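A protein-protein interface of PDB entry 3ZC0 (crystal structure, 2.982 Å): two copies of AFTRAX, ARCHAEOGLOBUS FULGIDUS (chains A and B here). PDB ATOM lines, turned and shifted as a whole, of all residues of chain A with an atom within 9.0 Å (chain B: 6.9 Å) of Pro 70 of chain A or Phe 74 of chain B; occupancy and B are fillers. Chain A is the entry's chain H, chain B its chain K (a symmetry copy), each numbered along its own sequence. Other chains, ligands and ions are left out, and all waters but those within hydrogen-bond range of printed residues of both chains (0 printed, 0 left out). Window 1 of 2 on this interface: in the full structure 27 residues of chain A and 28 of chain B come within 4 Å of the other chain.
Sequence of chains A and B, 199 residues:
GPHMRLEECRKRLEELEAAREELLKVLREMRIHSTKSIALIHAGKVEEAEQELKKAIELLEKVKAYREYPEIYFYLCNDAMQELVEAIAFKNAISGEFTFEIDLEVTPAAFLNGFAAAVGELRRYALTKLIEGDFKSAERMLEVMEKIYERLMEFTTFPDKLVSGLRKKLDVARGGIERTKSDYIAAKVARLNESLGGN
Pro 70 of chain B touches its own counterpart, Pro 70 of chain A.
Pro 70 of chain A touches Phe 74 of chain B, and with the chains exchanged Phe 74 of chain A touches Pro 70 of chain B.
Glu 71 of chain A touches Phe 74 of chain B, and with the chains exchanged Phe 74 of chain A touches Glu 71 of chain B.
Tyr 75 of chain B touches its own counterpart, Tyr 75 of chain A.
Positions printed for both chains: 23, 66, 67, 69, 70, 71, 72, 73, 74, 75 and 76.
Among the printed residues, pairs that only touch across the chains: Phe 74 of chain A with Pro 70 of chain B, Pro 70 of chain A with Phe 74 of chain B, Tyr 75 of chain A with Tyr 75 of chain B, Glu 71 of chain A with Phe 74 of chain B, Phe 74 of chain A with Glu 71 of chain B and Pro 70 of chain A with Pro 70 of chain B.
Arg 12 of chain A touches none of the printed residues of chain B.
Of chain B, only Pro 70 (3.97 Å) and Phe 74 (3.3 Å) come within 4 Å of Pro 70 of chain A.
Printed residues of chain B within 4 Å of Glu 71 of chain A: Phe 74.
Of the printed residues of chain B, Phe 74 of chain A touches Pro 70 (3.3 Å) and Glu 71 (3.9 Å).
Of the printed residues of chain B, Tyr 75 of chain A touches Tyr 75 (3.3 Å).
Tyr 69 of chain B touches none of the printed residues of chain A.
Of the printed residues of chain A, Pro 70 of chain B touches Pro 70 and Phe 74.
Of the printed residues of chain A, Glu 71 of chain B touches Phe 74.
The nearest residue of chain B that does not touch Pro 70 of chain A is Glu 71 of chain B (6.0 Å).
Of the 16 printed residues of chain A, 4 touch a printed residue of chain B.
Hydrophobic or aromatic side chains of chain A that line the printed part of chain B: Pro 70, Phe 74 and Tyr 75.
OE1 of Glu 71 of chain A is in salt-bridge range of NH2 of Arg 12 of chain A, 2.5 Å away.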
ATOM      1  N   ARG A  12     -22.047  -7.560 -18.945  1.00  0.00           N
ATOM      2  CA  ARG A  12     -22.232  -8.913 -19.460  1.00  0.00           C
ATOM      3  C   ARG A  12     -23.698  -9.319 -19.445  1.00  0.00           C
ATOM      4  O   ARG A  12     -24.168  -9.997 -20.347  1.00  0.00           O
ATOM      5  CB  ARG A  12     -21.397  -9.911 -18.661  1.00  0.00           C
ATOM      6  CG  ARG A  12     -21.387 -11.325 -19.226  1.00  0.00           C
ATOM      7  CD  ARG A  12     -20.948 -11.385 -20.695  1.00  0.00           C
ATOM      8  NE  ARG A  12     -20.935 -12.758 -21.191  1.00  0.00           N
ATOM      9  CZ  ARG A  12     -20.621 -13.096 -22.434  1.00  0.00           C
ATOM     10  NH1 ARG A  12     -20.301 -12.159 -23.308  1.00  0.00           N
ATOM     11  NH2 ARG A  12     -20.633 -14.368 -22.806  1.00  0.00           N
ATOM     12  N   LEU A  16     -25.924 -10.438 -22.560  1.00  0.00           N
ATOM     13  CA  LEU A  16     -26.617 -11.714 -22.528  1.00  0.00           C
ATOM     14  C   LEU A  16     -28.104 -11.519 -22.750  1.00  0.00           C
ATOM     15  O   LEU A  16     -28.709 -12.286 -23.469  1.00  0.00           O
ATOM     16  CB  LEU A  16     -26.328 -12.478 -21.235  1.00  0.00           C
ATOM     17  CG  LEU A  16     -24.939 -13.116 -21.309  1.00  0.00           C
ATOM     18  CD1 LEU A  16     -24.307 -13.415 -19.950  1.00  0.00           C
ATOM     19  CD2 LEU A  16     -25.037 -14.375 -22.134  1.00  0.00           C
ATOM     20  N   ALA A  19     -28.689 -10.659 -26.481  1.00  0.00           N
ATOM     21  CA  ALA A  19     -28.398 -11.848 -27.255  1.00  0.00           C
ATOM     22  C   ALA A  19     -29.576 -12.789 -27.132  1.00  0.00           C
ATOM     23  O   ALA A  19     -30.190 -13.116 -28.127  1.00  0.00           O
ATOM     24  CB  ALA A  19     -27.101 -12.505 -26.784  1.00  0.00           C
ATOM     25  N   LEU A  23     -31.314 -14.186 -30.488  1.00  0.00           N
ATOM     26  CA  LEU A  23     -31.260 -15.633 -30.623  1.00  0.00           C
ATOM     27  C   LEU A  23     -32.649 -16.228 -30.629  1.00  0.00           C
ATOM     28  O   LEU A  23     -32.989 -16.972 -31.530  1.00  0.00           O
ATOM     29  CB  LEU A  23     -30.467 -16.238 -29.466  1.00  0.00           C
ATOM     30  CG  LEU A  23     -29.476 -17.352 -29.786  1.00  0.00           C
ATOM     31  CD1 LEU A  23     -29.399 -18.284 -28.606  1.00  0.00           C
ATOM     32  CD2 LEU A  23     -29.869 -18.101 -31.041  1.00  0.00           C
ATOM     33  N   ALA A  65     -23.845 -17.555 -34.919  1.00  0.00           N
ATOM     34  CA  ALA A  65     -23.156 -16.378 -34.395  1.00  0.00           C
ATOM     35  C   ALA A  65     -23.000 -16.440 -32.880  1.00  0.00           C
ATOM     36  O   ALA A  65     -21.939 -16.144 -32.325  1.00  0.00           O
ATOM     37  CB  ALA A  65     -23.916 -15.116 -34.779  1.00  0.00           C
ATOM     38  N   TYR A  66     -24.069 -16.849 -32.217  1.00  0.00           N
ATOM     39  CA  TYR A  66     -24.200 -16.637 -30.788  1.00  0.00           C
ATOM     40  C   TYR A  66     -23.470 -17.623 -29.888  1.00  0.00           C
ATOM     41  O   TYR A  66     -23.691 -17.614 -28.684  1.00  0.00           O
ATOM     42  CB  TYR A  66     -25.675 -16.607 -30.415  1.00  0.00           C
ATOM     43  CG  TYR A  66     -26.417 -15.437 -31.003  1.00  0.00           C
ATOM     44  CD1 TYR A  66     -26.837 -15.447 -32.327  1.00  0.00           C
ATOM     45  CD2 TYR A  66     -26.692 -14.316 -30.234  1.00  0.00           C
ATOM     46  CE1 TYR A  66     -27.520 -14.369 -32.865  1.00  0.00           C
ATOM     47  CE2 TYR A  66     -27.375 -13.233 -30.761  1.00  0.00           C
ATOM     48  CZ  TYR A  66     -27.791 -13.264 -32.075  1.00  0.00           C
ATOM     49  OH  TYR A  66     -28.471 -12.190 -32.602  1.00  0.00           O
ATOM     50  N   ARG A  67     -22.598 -18.464 -30.435  1.00  0.00           N
ATOM     51  CA  ARG A  67     -21.845 -19.367 -29.562  1.00  0.00           C
ATOM     52  C   ARG A  67     -20.875 -18.602 -28.672  1.00  0.00           C
ATOM     53  O   ARG A  67     -20.308 -19.171 -27.737  1.00  0.00           O
ATOM     54  CB  ARG A  67     -21.096 -20.451 -30.339  1.00  0.00           C
ATOM     55  CG  ARG A  67     -21.056 -20.257 -31.840  1.00  0.00           C
ATOM     56  CD  ARG A  67     -21.939 -21.281 -32.544  1.00  0.00           C
ATOM     57  NE  ARG A  67     -21.540 -22.664 -32.278  1.00  0.00           N
ATOM     58  CZ  ARG A  67     -20.502 -23.269 -32.849  1.00  0.00           C
ATOM     59  NH1 ARG A  67     -19.741 -22.601 -33.704  1.00  0.00           N
ATOM     60  NH2 ARG A  67     -20.220 -24.537 -32.555  1.00  0.00           N
ATOM     61  N   GLU A  68     -20.688 -17.312 -28.951  1.00  0.00           N
ATOM     62  CA  GLU A  68     -19.851 -16.485 -28.088  1.00  0.00           C
ATOM     63  C   GLU A  68     -20.594 -16.204 -26.789  1.00  0.00           C
ATOM     64  O   GLU A  68     -20.078 -15.559 -25.879  1.00  0.00           O
ATOM     65  CB  GLU A  68     -19.421 -15.181 -28.778  1.00  0.00           C
ATOM     66  CG  GLU A  68     -20.536 -14.185 -29.036  1.00  0.00           C
ATOM     67  CD  GLU A  68     -20.012 -12.802 -29.389  1.00  0.00           C
ATOM     68  OE1 GLU A  68     -19.557 -12.085 -28.471  1.00  0.00           O
ATOM     69  OE2 GLU A  68     -20.059 -12.430 -30.582  1.00  0.00           O
ATOM     70  N   TYR A  69     -21.815 -16.708 -26.708  1.00  0.00           N
ATOM     71  CA  TYR A  69     -22.575 -16.652 -25.482  1.00  0.00           C
ATOM     72  C   TYR A  69     -22.918 -18.068 -25.050  1.00  0.00           C
ATOM     73  O   TYR A  69     -24.069 -18.487 -25.138  1.00  0.00           O
ATOM     74  CB  TYR A  69     -23.841 -15.822 -25.692  1.00  0.00           C
ATOM     75  CG  TYR A  69     -23.564 -14.458 -26.267  1.00  0.00           C
ATOM     76  CD1 TYR A  69     -22.816 -13.525 -25.557  1.00  0.00           C
ATOM     77  CD2 TYR A  69     -24.044 -14.098 -27.520  1.00  0.00           C
ATOM     78  CE1 TYR A  69     -22.556 -12.262 -26.077  1.00  0.00           C
ATOM     79  CE2 TYR A  69     -23.789 -12.832 -28.052  1.00  0.00           C
ATOM     80  CZ  TYR A  69     -23.044 -11.918 -27.323  1.00  0.00           C
ATOM     81  OH  TYR A  69     -22.785 -10.663 -27.831  1.00  0.00           O
ATOM     82  N   PRO A  70     -21.914 -18.817 -24.573  1.00  0.00           N
ATOM     83  CA  PRO A  70     -22.174 -20.209 -24.197  1.00  0.00           C
ATOM     84  C   PRO A  70     -23.061 -20.290 -22.958  1.00  0.00           C
ATOM     85  O   PRO A  70     -23.726 -21.307 -22.758  1.00  0.00           O
ATOM     86  CB  PRO A  70     -20.770 -20.763 -23.897  1.00  0.00           C
ATOM     87  CG  PRO A  70     -19.810 -19.754 -24.416  1.00  0.00           C
ATOM     88  CD  PRO A  70     -20.518 -18.443 -24.299  1.00  0.00           C
ATOM     89  N   GLU A  71     -23.075 -19.221 -22.161  1.00  0.00           N
ATOM     90  CA  GLU A  71     -23.906 -19.134 -20.965  1.00  0.00           C
ATOM     91  C   GLU A  71     -25.389 -19.290 -21.287  1.00  0.00           C
ATOM     92  O   GLU A  71     -26.192 -19.584 -20.407  1.00  0.00           O
ATOM     93  CB  GLU A  71     -23.671 -17.804 -20.255  1.00  0.00           C
ATOM     94  CG  GLU A  71     -22.257 -17.633 -19.718  1.00  0.00           C
ATOM     95  CD  GLU A  71     -21.599 -16.369 -20.230  1.00  0.00           C
ATOM     96  OE1 GLU A  71     -21.767 -16.088 -21.436  1.00  0.00           O
ATOM     97  OE2 GLU A  71     -20.931 -15.657 -19.436  1.00  0.00           O
ATOM     98  N   ILE A  72     -25.746 -19.058 -22.547  1.00  0.00           N
ATOM     99  CA  ILE A  72     -27.075 -19.373 -23.054  1.00  0.00           C
ATOM    100  C   ILE A  72     -26.900 -20.349 -24.235  1.00  0.00           C
ATOM    101  O   ILE A  72     -26.434 -21.472 -24.047  1.00  0.00           O
ATOM    102  CB  ILE A  72     -27.853 -18.090 -23.427  1.00  0.00           C
ATOM    103  CG1 ILE A  72     -26.957 -17.097 -24.162  1.00  0.00           C
ATOM    104  CG2 ILE A  72     -28.317 -17.364 -22.178  1.00  0.00           C
ATOM    105  CD1 ILE A  72     -27.726 -15.928 -24.719  1.00  0.00           C
ATOM    106  N   TYR A  73     -27.240 -19.919 -25.439  1.00  0.00           N
ATOM    107  CA  TYR A  73     -27.000 -20.692 -26.670  1.00  0.00           C
ATOM    108  C   TYR A  73     -27.533 -22.117 -26.677  1.00  0.00           C
ATOM    109  O   TYR A  73     -28.574 -22.385 -27.261  1.00  0.00           O
ATOM    110  CB  TYR A  73     -25.526 -20.701 -27.093  1.00  0.00           C
ATOM    111  CG  TYR A  73     -25.360 -21.231 -28.505  1.00  0.00           C
ATOM    112  CD1 TYR A  73     -25.671 -20.440 -29.608  1.00  0.00           C
ATOM    113  CD2 TYR A  73     -24.931 -22.528 -28.738  1.00  0.00           C
ATOM    114  CE1 TYR A  73     -25.535 -20.918 -30.901  1.00  0.00           C
ATOM    115  CE2 TYR A  73     -24.792 -23.013 -30.025  1.00  0.00           C
ATOM    116  CZ  TYR A  73     -25.099 -22.205 -31.101  1.00  0.00           C
ATOM    117  OH  TYR A  73     -24.968 -22.690 -32.381  1.00  0.00           O
ATOM    118  N   PHE A  74     -26.810 -23.030 -26.046  1.00  0.00           N
ATOM    119  CA  PHE A  74     -27.186 -24.440 -26.059  1.00  0.00           C
ATOM    120  C   PHE A  74     -28.584 -24.653 -25.520  1.00  0.00           C
ATOM    121  O   PHE A  74     -29.470 -25.200 -26.235  1.00  0.00           O
ATOM    122  CB  PHE A  74     -26.151 -25.257 -25.289  1.00  0.00           C
ATOM    123  CG  PHE A  74     -24.800 -25.142 -25.874  1.00  0.00           C
ATOM    124  CD1 PHE A  74     -24.418 -25.954 -26.916  1.00  0.00           C
ATOM    125  CD2 PHE A  74     -23.950 -24.139 -25.463  1.00  0.00           C
ATOM    126  CE1 PHE A  74     -23.184 -25.811 -27.499  1.00  0.00           C
ATOM    127  CE2 PHE A  74     -22.720 -23.987 -26.043  1.00  0.00           C
ATOM    128  CZ  PHE A  74     -22.330 -24.829 -27.056  1.00  0.00           C
ATOM    129  N   TYR A  75     -28.770 -24.189 -24.282  1.00  0.00           N
ATOM    130  CA  TYR A  75     -30.058 -24.233 -23.608  1.00  0.00           C
ATOM    131  C   TYR A  75     -31.164 -23.704 -24.517  1.00  0.00           C
ATOM    132  O   TYR A  75     -32.229 -24.312 -24.642  1.00  0.00           O
ATOM    133  CB  TYR A  75     -30.011 -23.443 -22.304  1.00  0.00           C
ATOM    134  CG  TYR A  75     -31.284 -23.535 -21.508  1.00  0.00           C
ATOM    135  CD1 TYR A  75     -32.338 -22.660 -21.742  1.00  0.00           C
ATOM    136  CD2 TYR A  75     -31.444 -24.505 -20.527  1.00  0.00           C
ATOM    137  CE1 TYR A  75     -33.521 -22.749 -21.018  1.00  0.00           C
ATOM    138  CE2 TYR A  75     -32.626 -24.601 -19.797  1.00  0.00           C
ATOM    139  CZ  TYR A  75     -33.657 -23.720 -20.047  1.00  0.00           C
ATOM    140  OH  TYR A  75     -34.827 -23.816 -19.329  1.00  0.00           O
ATOM    141  N   LEU A  76     -30.892 -22.589 -25.181  1.00  0.00           N
ATOM    142  CA  LEU A  76     -31.866 -21.974 -26.078  1.00  0.00           C
ATOM    143  C   LEU A  76     -32.029 -22.685 -27.409  1.00  0.00           C
ATOM    144  O   LEU A  76     -33.130 -22.743 -27.961  1.00  0.00           O
ATOM    145  CB  LEU A  76     -31.461 -20.533 -26.342  1.00  0.00           C
ATOM    146  CG  LEU A  76     -31.611 -19.690 -25.087  1.00  0.00           C
ATOM    147  CD1 LEU A  76     -31.017 -18.307 -25.291  1.00  0.00           C
ATOM    148  CD2 LEU A  76     -33.093 -19.633 -24.762  1.00  0.00           C
ATOM    149  N   LEU B  23     -15.377 -33.229 -13.840  1.00  0.00           N
ATOM    150  CA  LEU B  23     -15.854 -31.903 -13.463  1.00  0.00           C
ATOM    151  C   LEU B  23     -16.632 -31.963 -12.161  1.00  0.00           C
ATOM    152  O   LEU B  23     -16.344 -31.203 -11.237  1.00  0.00           O
ATOM    153  CB  LEU B  23     -16.768 -31.332 -14.546  1.00  0.00           C
ATOM    154  CG  LEU B  23     -16.835 -29.813 -14.756  1.00  0.00           C
ATOM    155  CD1 LEU B  23     -18.279 -29.345 -15.009  1.00  0.00           C
ATOM    156  CD2 LEU B  23     -16.170 -29.040 -13.625  1.00  0.00           C
ATOM    157  N   TYR B  66     -12.456 -27.059 -17.647  1.00  0.00           N
ATOM    158  CA  TYR B  66     -13.521 -27.691 -18.440  1.00  0.00           C
ATOM    159  C   TYR B  66     -14.434 -26.748 -19.222  1.00  0.00           C
ATOM    160  O   TYR B  66     -15.527 -27.146 -19.624  1.00  0.00           O
ATOM    161  CB  TYR B  66     -14.383 -28.611 -17.573  1.00  0.00           C
ATOM    162  CG  TYR B  66     -13.610 -29.727 -16.917  1.00  0.00           C
ATOM    163  CD1 TYR B  66     -12.897 -29.505 -15.746  1.00  0.00           C
ATOM    164  CD2 TYR B  66     -13.584 -31.006 -17.468  1.00  0.00           C
ATOM    165  CE1 TYR B  66     -12.189 -30.521 -15.135  1.00  0.00           C
ATOM    166  CE2 TYR B  66     -12.864 -32.037 -16.864  1.00  0.00           C
ATOM    167  CZ  TYR B  66     -12.169 -31.780 -15.696  1.00  0.00           C
ATOM    168  OH  TYR B  66     -11.447 -32.769 -15.071  1.00  0.00           O
ATOM    169  N   ARG B  67     -13.996 -25.515 -19.448  1.00  0.00           N
ATOM    170  CA  ARG B  67     -14.801 -24.568 -20.219  1.00  0.00           C
ATOM    171  C   ARG B  67     -14.887 -24.985 -21.686  1.00  0.00           C
ATOM    172  O   ARG B  67     -15.714 -24.461 -22.422  1.00  0.00           O
ATOM    173  CB  ARG B  67     -14.242 -23.136 -20.118  1.00  0.00           C
ATOM    174  CG  ARG B  67     -14.992 -22.203 -19.156  1.00  0.00           C
ATOM    175  CD  ARG B  67     -14.669 -20.724 -19.409  1.00  0.00           C
ATOM    176  NE  ARG B  67     -13.230 -20.470 -19.424  1.00  0.00           N
ATOM    177  CZ  ARG B  67     -12.513 -20.153 -18.349  1.00  0.00           C
ATOM    178  NH1 ARG B  67     -13.099 -20.046 -17.164  1.00  0.00           N
ATOM    179  NH2 ARG B  67     -11.208 -19.944 -18.457  1.00  0.00           N
ATOM    180  N   TYR B  69     -15.999 -27.485 -22.807  1.00  0.00           N
ATOM    181  CA  TYR B  69     -17.241 -28.210 -22.950  1.00  0.00           C
ATOM    182  C   TYR B  69     -18.383 -27.263 -22.575  1.00  0.00           C
ATOM    183  O   TYR B  69     -18.982 -27.396 -21.499  1.00  0.00           O
ATOM    184  CB  TYR B  69     -17.232 -29.420 -22.021  1.00  0.00           C
ATOM    185  CG  TYR B  69     -16.046 -30.339 -22.217  1.00  0.00           C
ATOM    186  CD1 TYR B  69     -15.912 -31.084 -23.374  1.00  0.00           C
ATOM    187  CD2 TYR B  69     -15.077 -30.477 -21.236  1.00  0.00           C
ATOM    188  CE1 TYR B  69     -14.848 -31.933 -23.555  1.00  0.00           C
ATOM    189  CE2 TYR B  69     -14.004 -31.329 -21.409  1.00  0.00           C
ATOM    190  CZ  TYR B  69     -13.899 -32.054 -22.575  1.00  0.00           C
ATOM    191  OH  TYR B  69     -12.845 -32.912 -22.776  1.00  0.00           O
ATOM    192  N   PRO B  70     -18.665 -26.277 -23.446  1.00  0.00           N
ATOM    193  CA  PRO B  70     -19.743 -25.315 -23.200  1.00  0.00           C
ATOM    194  C   PRO B  70     -21.060 -25.998 -22.814  1.00  0.00           C
ATOM    195  O   PRO B  70     -21.553 -25.737 -21.722  1.00  0.00           O
ATOM    196  CB  PRO B  70     -19.859 -24.574 -24.535  1.00  0.00           C
ATOM    197  CG  PRO B  70     -18.514 -24.653 -25.122  1.00  0.00           C
ATOM    198  CD  PRO B  70     -17.979 -26.005 -24.721  1.00  0.00           C
ATOM    199  N   GLU B  71     -21.610 -26.856 -23.666  1.00  0.00           N
ATOM    200  CA  GLU B  71     -22.695 -27.733 -23.230  1.00  0.00           C
ATOM    201  C   GLU B  71     -22.168 -28.498 -22.019  1.00  0.00           C
ATOM    202  O   GLU B  71     -20.983 -28.775 -21.958  1.00  0.00           O
ATOM    203  CB  GLU B  71     -23.138 -28.673 -24.359  1.00  0.00           C
ATOM    204  CG  GLU B  71     -22.224 -29.861 -24.651  1.00  0.00           C
ATOM    205  CD  GLU B  71     -20.987 -29.501 -25.455  1.00  0.00           C
ATOM    206  OE1 GLU B  71     -20.143 -28.747 -24.937  1.00  0.00           O
ATOM    207  OE2 GLU B  71     -20.844 -29.994 -26.595  1.00  0.00           O
ATOM    208  N   ILE B  72     -23.030 -28.849 -21.071  1.00  0.00           N
ATOM    209  CA  ILE B  72     -22.596 -29.033 -19.667  1.00  0.00           C
ATOM    210  C   ILE B  72     -21.921 -27.740 -19.156  1.00  0.00           C
ATOM    211  O   ILE B  72     -22.452 -26.660 -19.407  1.00  0.00           O
ATOM    212  CB  ILE B  72     -21.879 -30.417 -19.328  1.00  0.00           C
ATOM    213  CG1 ILE B  72     -20.385 -30.471 -19.648  1.00  0.00           C
ATOM    214  CG2 ILE B  72     -22.560 -31.561 -20.057  1.00  0.00           C
ATOM    215  CD1 ILE B  72     -19.710 -31.681 -19.076  1.00  0.00           C
ATOM    216  N   TYR B  73     -20.785 -27.823 -18.469  1.00  0.00           N
ATOM    217  CA  TYR B  73     -20.145 -26.673 -17.786  1.00  0.00           C
ATOM    218  C   TYR B  73     -21.077 -25.685 -17.068  1.00  0.00           C
ATOM    219  O   TYR B  73     -21.314 -25.817 -15.870  1.00  0.00           O
ATOM    220  CB  TYR B  73     -19.179 -25.900 -18.688  1.00  0.00           C
ATOM    221  CG  TYR B  73     -18.218 -25.040 -17.882  1.00  0.00           C
ATOM    222  CD1 TYR B  73     -17.075 -25.587 -17.309  1.00  0.00           C
ATOM    223  CD2 TYR B  73     -18.463 -23.691 -17.674  1.00  0.00           C
ATOM    224  CE1 TYR B  73     -16.194 -24.813 -16.562  1.00  0.00           C
ATOM    225  CE2 TYR B  73     -17.586 -22.907 -16.933  1.00  0.00           C
ATOM    226  CZ  TYR B  73     -16.458 -23.475 -16.376  1.00  0.00           C
ATOM    227  OH  TYR B  73     -15.593 -22.694 -15.640  1.00  0.00           O
ATOM    228  N   PHE B  74     -21.591 -24.695 -17.800  1.00  0.00           N
ATOM    229  CA  PHE B  74     -22.508 -23.686 -17.230  1.00  0.00           C
ATOM    230  C   PHE B  74     -23.762 -24.250 -16.517  1.00  0.00           C
ATOM    231  O   PHE B  74     -24.265 -23.620 -15.574  1.00  0.00           O
ATOM    232  CB  PHE B  74     -22.916 -22.633 -18.286  1.00  0.00           C
ATOM    233  CG  PHE B  74     -21.749 -21.912 -18.893  1.00  0.00           C
ATOM    234  CD1 PHE B  74     -21.025 -21.004 -18.144  1.00  0.00           C
ATOM    235  CD2 PHE B  74     -21.350 -22.172 -20.190  1.00  0.00           C
ATOM    236  CE1 PHE B  74     -19.936 -20.363 -18.676  1.00  0.00           C
ATOM    237  CE2 PHE B  74     -20.267 -21.525 -20.723  1.00  0.00           C
ATOM    238  CZ  PHE B  74     -19.563 -20.615 -19.966  1.00  0.00           C
ATOM    239  N   TYR B  75     -24.245 -25.421 -16.966  1.00  0.00           N
ATOM    240  CA  TYR B  75     -25.402 -26.113 -16.370  1.00  0.00           C
ATOM    241  C   TYR B  75     -25.117 -26.599 -14.983  1.00  0.00           C
ATOM    242  O   TYR B  75     -26.041 -27.019 -14.288  1.00  0.00           O
ATOM    243  CB  TYR B  75     -25.772 -27.381 -17.139  1.00  0.00           C
ATOM    244  CG  TYR B  75     -26.648 -27.205 -18.352  1.00  0.00           C
ATOM    245  CD1 TYR B  75     -26.227 -26.442 -19.446  1.00  0.00           C
ATOM    246  CD2 TYR B  75     -27.887 -27.827 -18.421  1.00  0.00           C
ATOM    247  CE1 TYR B  75     -27.029 -26.292 -20.566  1.00  0.00           C
ATOM    248  CE2 TYR B  75     -28.694 -27.686 -19.536  1.00  0.00           C
ATOM    249  CZ  TYR B  75     -28.263 -26.919 -20.600  1.00  0.00           C
ATOM    250  OH  TYR B  75     -29.078 -26.783 -21.699  1.00  0.00           O
ATOM    251  N   LEU B  76     -23.844 -26.604 -14.594  1.00  0.00           N
ATOM    252  CA  LEU B  76     -23.484 -27.278 -13.353  1.00  0.00           C
ATOM    253  C   LEU B  76     -22.294 -26.710 -12.602  1.00  0.00           C
ATOM    254  O   LEU B  76     -21.773 -27.340 -11.686  1.00  0.00           O
ATOM    255  CB  LEU B  76     -23.331 -28.790 -13.568  1.00  0.00           C
ATOM    256  CG  LEU B  76     -22.250 -29.431 -14.429  1.00  0.00           C
ATOM    257  CD1 LEU B  76     -22.438 -30.935 -14.347  1.00  0.00           C
ATOM    258  CD2 LEU B  76     -22.296 -28.971 -15.882  1.00  0.00           C
ATOM    259  N   CYS B  77     -21.881 -25.502 -12.957  1.00  0.00           N
ATOM    260  CA  CYS B  77     -20.777 -24.863 -12.259  1.00  0.00           C
ATOM    261  C   CYS B  77     -21.324 -24.058 -11.101  1.00  0.00           C
ATOM    262  O   CYS B  77     -20.823 -24.141  -9.960  1.00  0.00           O
ATOM    263  CB  CYS B  77     -20.013 -23.959 -13.217  1.00  0.00           C
ATOM    264  SG  CYS B  77     -18.686 -24.822 -14.090  1.00  0.00           S
ATOM    265  N   ASN B  78     -22.388 -23.316 -11.419  1.00  0.00           N
ATOM    266  CA  ASN B  78     -23.026 -22.356 -10.527  1.00  0.00           C
ATOM    267  C   ASN B  78     -22.894 -22.571  -9.027  1.00  0.00           C
ATOM    268  O   ASN B  78     -22.233 -21.775  -8.340  1.00  0.00           O
ATOM    269  CB  ASN B  78     -24.491 -22.213 -10.872  1.00  0.00           C
ATOM    270  CG  ASN B  78     -24.860 -20.787 -11.116  1.00  0.00           C
ATOM    271  OD1 ASN B  78     -25.633 -20.184 -10.353  1.00  0.00           O
ATOM    272  ND2 ASN B  78     -24.264 -20.201 -12.166  1.00  0.00           N
ATOM    273  N   MET B  81     -19.408 -22.414  -7.675  1.00  0.00           N
ATOM    274  CA  MET B  81     -18.974 -21.034  -7.861  1.00  0.00           C
ATOM    275  C   MET B  81     -19.621 -20.102  -6.831  1.00  0.00           C
ATOM    276  O   MET B  81     -18.914 -19.345  -6.140  1.00  0.00           O
ATOM    277  CB  MET B  81     -19.250 -20.572  -9.294  1.00  0.00           C
ATOM    278  CG  MET B  81     -18.343 -21.205 -10.334  1.00  0.00           C
ATOM    279  SD  MET B  81     -18.608 -20.492 -11.958  1.00  0.00           S
ATOM    280  CE  MET B  81     -17.312 -21.296 -12.911  1.00  0.00           C
ATOM    281  N   THR B 107     -19.421 -17.036 -13.151  1.00  0.00           N
ATOM    282  CA  THR B 107     -20.539 -16.463 -13.911  1.00  0.00           C
ATOM    283  C   THR B 107     -21.231 -15.338 -13.134  1.00  0.00           C
ATOM    284  O   THR B 107     -21.288 -15.384 -11.900  1.00  0.00           O
ATOM    285  CB  THR B 107     -21.572 -17.540 -14.348  1.00  0.00           C
ATOM    286  OG1 THR B 107     -22.391 -17.925 -13.232  1.00  0.00           O
ATOM    287  CG2 THR B 107     -20.856 -18.748 -14.899  1.00  0.00           C
